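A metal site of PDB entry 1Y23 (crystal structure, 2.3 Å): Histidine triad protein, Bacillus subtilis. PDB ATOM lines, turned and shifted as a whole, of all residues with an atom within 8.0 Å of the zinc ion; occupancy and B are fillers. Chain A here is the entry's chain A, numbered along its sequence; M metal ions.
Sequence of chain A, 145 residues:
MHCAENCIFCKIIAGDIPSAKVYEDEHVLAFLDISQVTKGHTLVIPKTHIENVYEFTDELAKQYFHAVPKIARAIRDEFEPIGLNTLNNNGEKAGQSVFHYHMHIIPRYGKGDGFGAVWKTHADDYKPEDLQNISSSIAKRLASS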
ATOM      1  N   GLU A   5       1.186 -17.548  10.740  1.00  0.00           N
ATOM      2  CA  GLU A   5       0.481 -18.612  11.515  1.00  0.00           C
ATOM      3  C   GLU A   5      -1.006 -18.621  11.101  1.00  0.00           C
ATOM      4  O   GLU A   5      -1.424 -17.906  10.182  1.00  0.00           O
ATOM      5  CB  GLU A   5       0.636 -18.336  13.015  1.00  0.00           C
ATOM      6  CG  GLU A   5       0.278 -19.507  13.957  1.00  0.00           C
ATOM      7  CD  GLU A   5       1.366 -20.593  14.040  1.00  0.00           C
ATOM      8  OE1 GLU A   5       1.621 -21.279  13.025  1.00  0.00           O
ATOM      9  OE2 GLU A   5       1.963 -20.759  15.131  1.00  0.00           O
ATOM     10  N   ASN A   6      -1.798 -19.450  11.777  1.00  0.00           N
ATOM     11  CA  ASN A   6      -3.242 -19.557  11.522  1.00  0.00           C
ATOM     12  C   ASN A   6      -4.004 -19.010  12.732  1.00  0.00           C
ATOM     13  O   ASN A   6      -5.154 -19.357  12.979  1.00  0.00           O
ATOM     14  CB  ASN A   6      -3.644 -21.017  11.297  1.00  0.00           C
ATOM     15  CG  ASN A   6      -3.080 -21.596  10.001  1.00  0.00           C
ATOM     16  OD1 ASN A   6      -3.202 -20.974   8.934  1.00  0.00           O
ATOM     17  ND2 ASN A   6      -2.474 -22.777  10.088  1.00  0.00           N
ATOM     18  N   CYS A   7      -3.321 -18.146  13.471  1.00  0.00           N
ATOM     19  CA  CYS A   7      -3.852 -17.528  14.680  1.00  0.00           C
ATOM     20  C   CYS A   7      -4.617 -16.249  14.411  1.00  0.00           C
ATOM     21  O   CYS A   7      -4.069 -15.285  13.872  1.00  0.00           O
ATOM     22  CB  CYS A   7      -2.698 -17.240  15.648  1.00  0.00           C
ATOM     23  SG  CYS A   7      -3.195 -16.336  17.113  1.00  0.00           S
ATOM     24  N   ILE A   8      -5.889 -16.223  14.791  1.00  0.00           N
ATOM     25  CA  ILE A   8      -6.713 -15.044  14.581  1.00  0.00           C
ATOM     26  C   ILE A   8      -6.163 -13.810  15.330  1.00  0.00           C
ATOM     27  O   ILE A   8      -6.236 -12.682  14.823  1.00  0.00           O
ATOM     28  CB  ILE A   8      -8.156 -15.310  15.032  1.00  0.00           C
ATOM     29  CG1 ILE A   8      -9.019 -14.061  14.875  1.00  0.00           C
ATOM     30  CG2 ILE A   8      -8.162 -15.784  16.479  1.00  0.00           C
ATOM     31  CD1 ILE A   8     -10.387 -14.191  15.519  1.00  0.00           C
ATOM     32  N   PHE A   9      -5.611 -14.022  16.533  1.00  0.00           N
ATOM     33  CA  PHE A   9      -5.053 -12.917  17.328  1.00  0.00           C
ATOM     34  C   PHE A   9      -3.775 -12.373  16.704  1.00  0.00           C
ATOM     35  O   PHE A   9      -3.501 -11.183  16.806  1.00  0.00           O
ATOM     36  CB  PHE A   9      -4.760 -13.371  18.766  1.00  0.00           C
ATOM     37  CG  PHE A   9      -5.974 -13.392  19.664  1.00  0.00           C
ATOM     38  CD1 PHE A   9      -7.246 -13.191  19.157  1.00  0.00           C
ATOM     39  CD2 PHE A   9      -5.837 -13.648  21.029  1.00  0.00           C
ATOM     40  CE1 PHE A   9      -8.374 -13.249  19.996  1.00  0.00           C
ATOM     41  CE2 PHE A   9      -6.945 -13.717  21.868  1.00  0.00           C
ATOM     42  CZ  PHE A   9      -8.215 -13.521  21.353  1.00  0.00           C
ATOM     43  N   CYS A  10      -2.993 -13.245  16.079  1.00  0.00           N
ATOM     44  CA  CYS A  10      -1.769 -12.774  15.449  1.00  0.00           C
ATOM     45  C   CYS A  10      -2.148 -11.914  14.255  1.00  0.00           C
ATOM     46  O   CYS A  10      -1.435 -10.972  13.911  1.00  0.00           O
ATOM     47  CB  CYS A  10      -0.901 -13.957  15.018  1.00  0.00           C
ATOM     48  SG  CYS A  10      -0.032 -14.720  16.403  1.00  0.00           S
ATOM     49  N   LYS A  11      -3.294 -12.229  13.658  1.00  0.00           N
ATOM     50  CA  LYS A  11      -3.771 -11.448  12.522  1.00  0.00           C
ATOM     51  C   LYS A  11      -4.252 -10.072  12.944  1.00  0.00           C
ATOM     52  O   LYS A  11      -4.181  -9.124  12.166  1.00  0.00           O
ATOM     53  CB  LYS A  11      -4.874 -12.226  11.801  1.00  0.00           C
ATOM     54  CG  LYS A  11      -4.316 -13.433  11.042  1.00  0.00           C
ATOM     55  CD  LYS A  11      -5.242 -13.893   9.943  1.00  0.00           C
ATOM     56  CE  LYS A  11      -4.588 -14.997   9.122  1.00  0.00           C
ATOM     57  NZ  LYS A  11      -3.310 -14.578   8.467  1.00  0.00           N
ATOM     58  N   ILE A  12      -4.749  -9.978  14.174  1.00  0.00           N
ATOM     59  CA  ILE A  12      -5.227  -8.709  14.736  1.00  0.00           C
ATOM     60  C   ILE A  12      -4.001  -7.849  15.041  1.00  0.00           C
ATOM     61  O   ILE A  12      -4.008  -6.641  14.807  1.00  0.00           O
ATOM     62  CB  ILE A  12      -6.017  -8.946  16.051  1.00  0.00           C
ATOM     63  CG1 ILE A  12      -7.348  -9.630  15.739  1.00  0.00           C
ATOM     64  CG2 ILE A  12      -6.220  -7.633  16.787  1.00  0.00           C
ATOM     65  CD1 ILE A  12      -8.237  -9.844  16.938  1.00  0.00           C
ATOM     66  N   ILE A  13      -2.964  -8.493  15.562  1.00  0.00           N
ATOM     67  CA  ILE A  13      -1.713  -7.843  15.920  1.00  0.00           C
ATOM     68  C   ILE A  13      -1.058  -7.288  14.659  1.00  0.00           C
ATOM     69  O   ILE A  13      -0.571  -6.158  14.641  1.00  0.00           O
ATOM     70  CB  ILE A  13      -0.740  -8.860  16.594  1.00  0.00           C
ATOM     71  CG1 ILE A  13      -1.346  -9.339  17.919  1.00  0.00           C
ATOM     72  CG2 ILE A  13       0.616  -8.233  16.839  1.00  0.00           C
ATOM     73  CD1 ILE A  13      -0.657 -10.548  18.486  1.00  0.00           C
ATOM     74  N   ILE A  45      -3.121  -9.204  25.321  1.00  0.00           N
ATOM     75  CA  ILE A  45      -2.289 -10.275  24.774  1.00  0.00           C
ATOM     76  C   ILE A  45      -0.882  -9.819  24.400  1.00  0.00           C
ATOM     77  O   ILE A  45      -0.638  -8.643  24.149  1.00  0.00           O
ATOM     78  CB  ILE A  45      -2.957 -10.900  23.513  1.00  0.00           C
ATOM     79  CG1 ILE A  45      -2.832  -9.942  22.320  1.00  0.00           C
ATOM     80  CG2 ILE A  45      -4.451 -11.160  23.764  1.00  0.00           C
ATOM     81  CD1 ILE A  45      -3.199 -10.565  20.963  1.00  0.00           C
ATOM     82  N   PRO A  46       0.089 -10.745  24.374  1.00  0.00           N
ATOM     83  CA  PRO A  46       1.477 -10.409  24.008  1.00  0.00           C
ATOM     84  C   PRO A  46       1.584 -10.412  22.499  1.00  0.00           C
ATOM     85  O   PRO A  46       1.017 -11.285  21.848  1.00  0.00           O
ATOM     86  CB  PRO A  46       2.273 -11.549  24.636  1.00  0.00           C
ATOM     87  CG  PRO A  46       1.339 -12.714  24.460  1.00  0.00           C
ATOM     88  CD  PRO A  46       0.030 -12.111  24.930  1.00  0.00           C
ATOM     89  N   LYS A  47       2.292  -9.444  21.943  1.00  0.00           N
ATOM     90  CA  LYS A  47       2.449  -9.408  20.497  1.00  0.00           C
ATOM     91  C   LYS A  47       3.153 -10.672  20.021  1.00  0.00           C
ATOM     92  O   LYS A  47       2.906 -11.141  18.919  1.00  0.00           O
ATOM     93  CB  LYS A  47       3.218  -8.154  20.071  1.00  0.00           C
ATOM     94  CG  LYS A  47       2.403  -6.895  20.226  1.00  0.00           C
ATOM     95  CD  LYS A  47       3.014  -5.721  19.500  1.00  0.00           C
ATOM     96  CE  LYS A  47       2.055  -4.545  19.495  1.00  0.00           C
ATOM     97  NZ  LYS A  47       2.590  -3.391  18.772  1.00  0.00           N
ATOM     98  N   THR A  48       4.029 -11.230  20.855  1.00  0.00           N
ATOM     99  CA  THR A  48       4.721 -12.456  20.473  1.00  0.00           C
ATOM    100  C   THR A  48       3.747 -13.624  20.665  1.00  0.00           C
ATOM    101  O   THR A  48       3.123 -13.763  21.723  1.00  0.00           O
ATOM    102  CB  THR A  48       5.953 -12.748  21.341  1.00  0.00           C
ATOM    103  OG1 THR A  48       6.866 -11.645  21.282  1.00  0.00           O
ATOM    104  CG2 THR A  48       6.646 -14.003  20.820  1.00  0.00           C
ATOM    105  N   HIS A  49       3.640 -14.469  19.655  1.00  0.00           N
ATOM    106  CA  HIS A  49       2.747 -15.600  19.702  1.00  0.00           C
ATOM    107  C   HIS A  49       3.173 -16.756  20.608  1.00  0.00           C
ATOM    108  O   HIS A  49       4.270 -17.315  20.462  1.00  0.00           O
ATOM    109  CB  HIS A  49       2.500 -16.160  18.304  1.00  0.00           C
ATOM    110  CG  HIS A  49       1.607 -17.360  18.284  1.00  0.00           C
ATOM    111  ND1 HIS A  49       0.241 -17.272  18.136  1.00  0.00           N
ATOM    112  CD2 HIS A  49       1.879 -18.681  18.447  1.00  0.00           C
ATOM    113  CE1 HIS A  49      -0.292 -18.479  18.201  1.00  0.00           C
ATOM    114  NE2 HIS A  49       0.681 -19.351  18.396  1.00  0.00           N
ATOM    115  N   ILE A  50       2.303 -17.089  21.547  1.00  0.00           N
ATOM    116  CA  ILE A  50       2.520 -18.219  22.449  1.00  0.00           C
ATOM    117  C   ILE A  50       1.108 -18.782  22.645  1.00  0.00           C
ATOM    118  O   ILE A  50       0.145 -18.029  22.782  1.00  0.00           O
ATOM    119  CB  ILE A  50       3.144 -17.808  23.806  1.00  0.00           C
ATOM    120  CG1 ILE A  50       2.388 -16.650  24.442  1.00  0.00           C
ATOM    121  CG2 ILE A  50       4.612 -17.454  23.598  1.00  0.00           C
ATOM    122  CD1 ILE A  50       2.885 -16.305  25.828  1.00  0.00           C
ATOM    123  N   GLU A  51       1.005 -20.108  22.605  1.00  0.00           N
ATOM    124  CA  GLU A  51      -0.279 -20.784  22.703  1.00  0.00           C
ATOM    125  C   GLU A  51      -0.969 -20.604  24.053  1.00  0.00           C
ATOM    126  O   GLU A  51      -2.192 -20.454  24.127  1.00  0.00           O
ATOM    127  CB  GLU A  51      -0.089 -22.265  22.408  1.00  0.00           C
ATOM    128  CG  GLU A  51      -1.354 -23.074  22.193  1.00  0.00           C
ATOM    129  CD  GLU A  51      -1.071 -24.568  22.080  1.00  0.00           C
ATOM    130  OE1 GLU A  51      -0.166 -24.936  21.309  1.00  0.00           O
ATOM    131  OE2 GLU A  51      -1.763 -25.362  22.763  1.00  0.00           O
ATOM    132  N   VAL A  98      -9.386 -19.403  21.479  1.00  0.00           N
ATOM    133  CA  VAL A  98      -8.337 -18.914  20.580  1.00  0.00           C
ATOM    134  C   VAL A  98      -7.023 -19.280  21.251  1.00  0.00           C
ATOM    135  O   VAL A  98      -6.752 -18.851  22.373  1.00  0.00           O
ATOM    136  CB  VAL A  98      -8.382 -17.384  20.413  1.00  0.00           C
ATOM    137  CG1 VAL A  98      -7.225 -16.918  19.536  1.00  0.00           C
ATOM    138  CG2 VAL A  98      -9.718 -16.971  19.816  1.00  0.00           C
ATOM    139  N   PHE A  99      -6.216 -20.078  20.551  1.00  0.00           N
ATOM    140  CA  PHE A  99      -4.950 -20.557  21.084  1.00  0.00           C
ATOM    141  C   PHE A  99      -3.735 -19.640  20.949  1.00  0.00           C
ATOM    142  O   PHE A  99      -2.763 -19.937  20.251  1.00  0.00           O
ATOM    143  CB  PHE A  99      -4.661 -21.943  20.503  1.00  0.00           C
ATOM    144  CG  PHE A  99      -5.556 -22.995  21.058  1.00  0.00           C
ATOM    145  CD1 PHE A  99      -5.175 -23.728  22.184  1.00  0.00           C
ATOM    146  CD2 PHE A  99      -6.811 -23.218  20.505  1.00  0.00           C
ATOM    147  CE1 PHE A  99      -6.027 -24.662  22.751  1.00  0.00           C
ATOM    148  CE2 PHE A  99      -7.676 -24.158  21.071  1.00  0.00           C
ATOM    149  CZ  PHE A  99      -7.278 -24.878  22.194  1.00  0.00           C
ATOM    150  N   HIS A 100      -3.827 -18.536  21.654  1.00  0.00           N
ATOM    151  CA  HIS A 100      -2.795 -17.523  21.722  1.00  0.00           C
ATOM    152  C   HIS A 100      -3.055 -16.944  23.106  1.00  0.00           C
ATOM    153  O   HIS A 100      -4.147 -16.442  23.373  1.00  0.00           O
ATOM    154  CB  HIS A 100      -3.015 -16.498  20.617  1.00  0.00           C
ATOM    155  CG  HIS A 100      -2.093 -15.318  20.682  1.00  0.00           C
ATOM    156  ND1 HIS A 100      -1.536 -14.756  19.558  1.00  0.00           N
ATOM    157  CD2 HIS A 100      -1.648 -14.584  21.737  1.00  0.00           C
ATOM    158  CE1 HIS A 100      -0.787 -13.728  19.911  1.00  0.00           C
ATOM    159  NE2 HIS A 100      -0.832 -13.603  21.228  1.00  0.00           N
ATOM    160  N   TYR A 101      -2.081 -17.063  23.997  1.00  0.00           N
ATOM    161  CA  TYR A 101      -2.248 -16.557  25.357  1.00  0.00           C
ATOM    162  C   TYR A 101      -2.972 -15.214  25.401  1.00  0.00           C
ATOM    163  O   TYR A 101      -2.669 -14.307  24.619  1.00  0.00           O
ATOM    164  CB  TYR A 101      -0.912 -16.427  26.064  1.00  0.00           C
ATOM    165  CG  TYR A 101      -1.093 -15.985  27.508  1.00  0.00           C
ATOM    166  CD1 TYR A 101      -1.245 -16.921  28.534  1.00  0.00           C
ATOM    167  CD2 TYR A 101      -1.187 -14.627  27.835  1.00  0.00           C
ATOM    168  CE1 TYR A 101      -1.502 -16.509  29.853  1.00  0.00           C
ATOM    169  CE2 TYR A 101      -1.444 -14.214  29.130  1.00  0.00           C
ATOM    170  CZ  TYR A 101      -1.609 -15.155  30.130  1.00  0.00           C
ATOM    171  OH  TYR A 101      -1.889 -14.740  31.404  1.00  0.00           O
HETATM  172 ZN    ZN M   1      -1.039 -15.932  17.826  1.00  0.00          ZN
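The backbone carbonyl oxygen of Pro 46 lies within hydrogen-bond range of a ring nitrogen (NE2) of His 100.
N of Phe 9 sits close to SG of Cys 7 (3.4 Å).
ND1 of His 49 is bound to the zinc ion.
The zinc ion is bound by SG of Cys 10.
ND1 of His 100 is bound to the zinc ion (2.2 Å).
SG of Cys 7 is bound to the zinc ion (2.3 Å).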
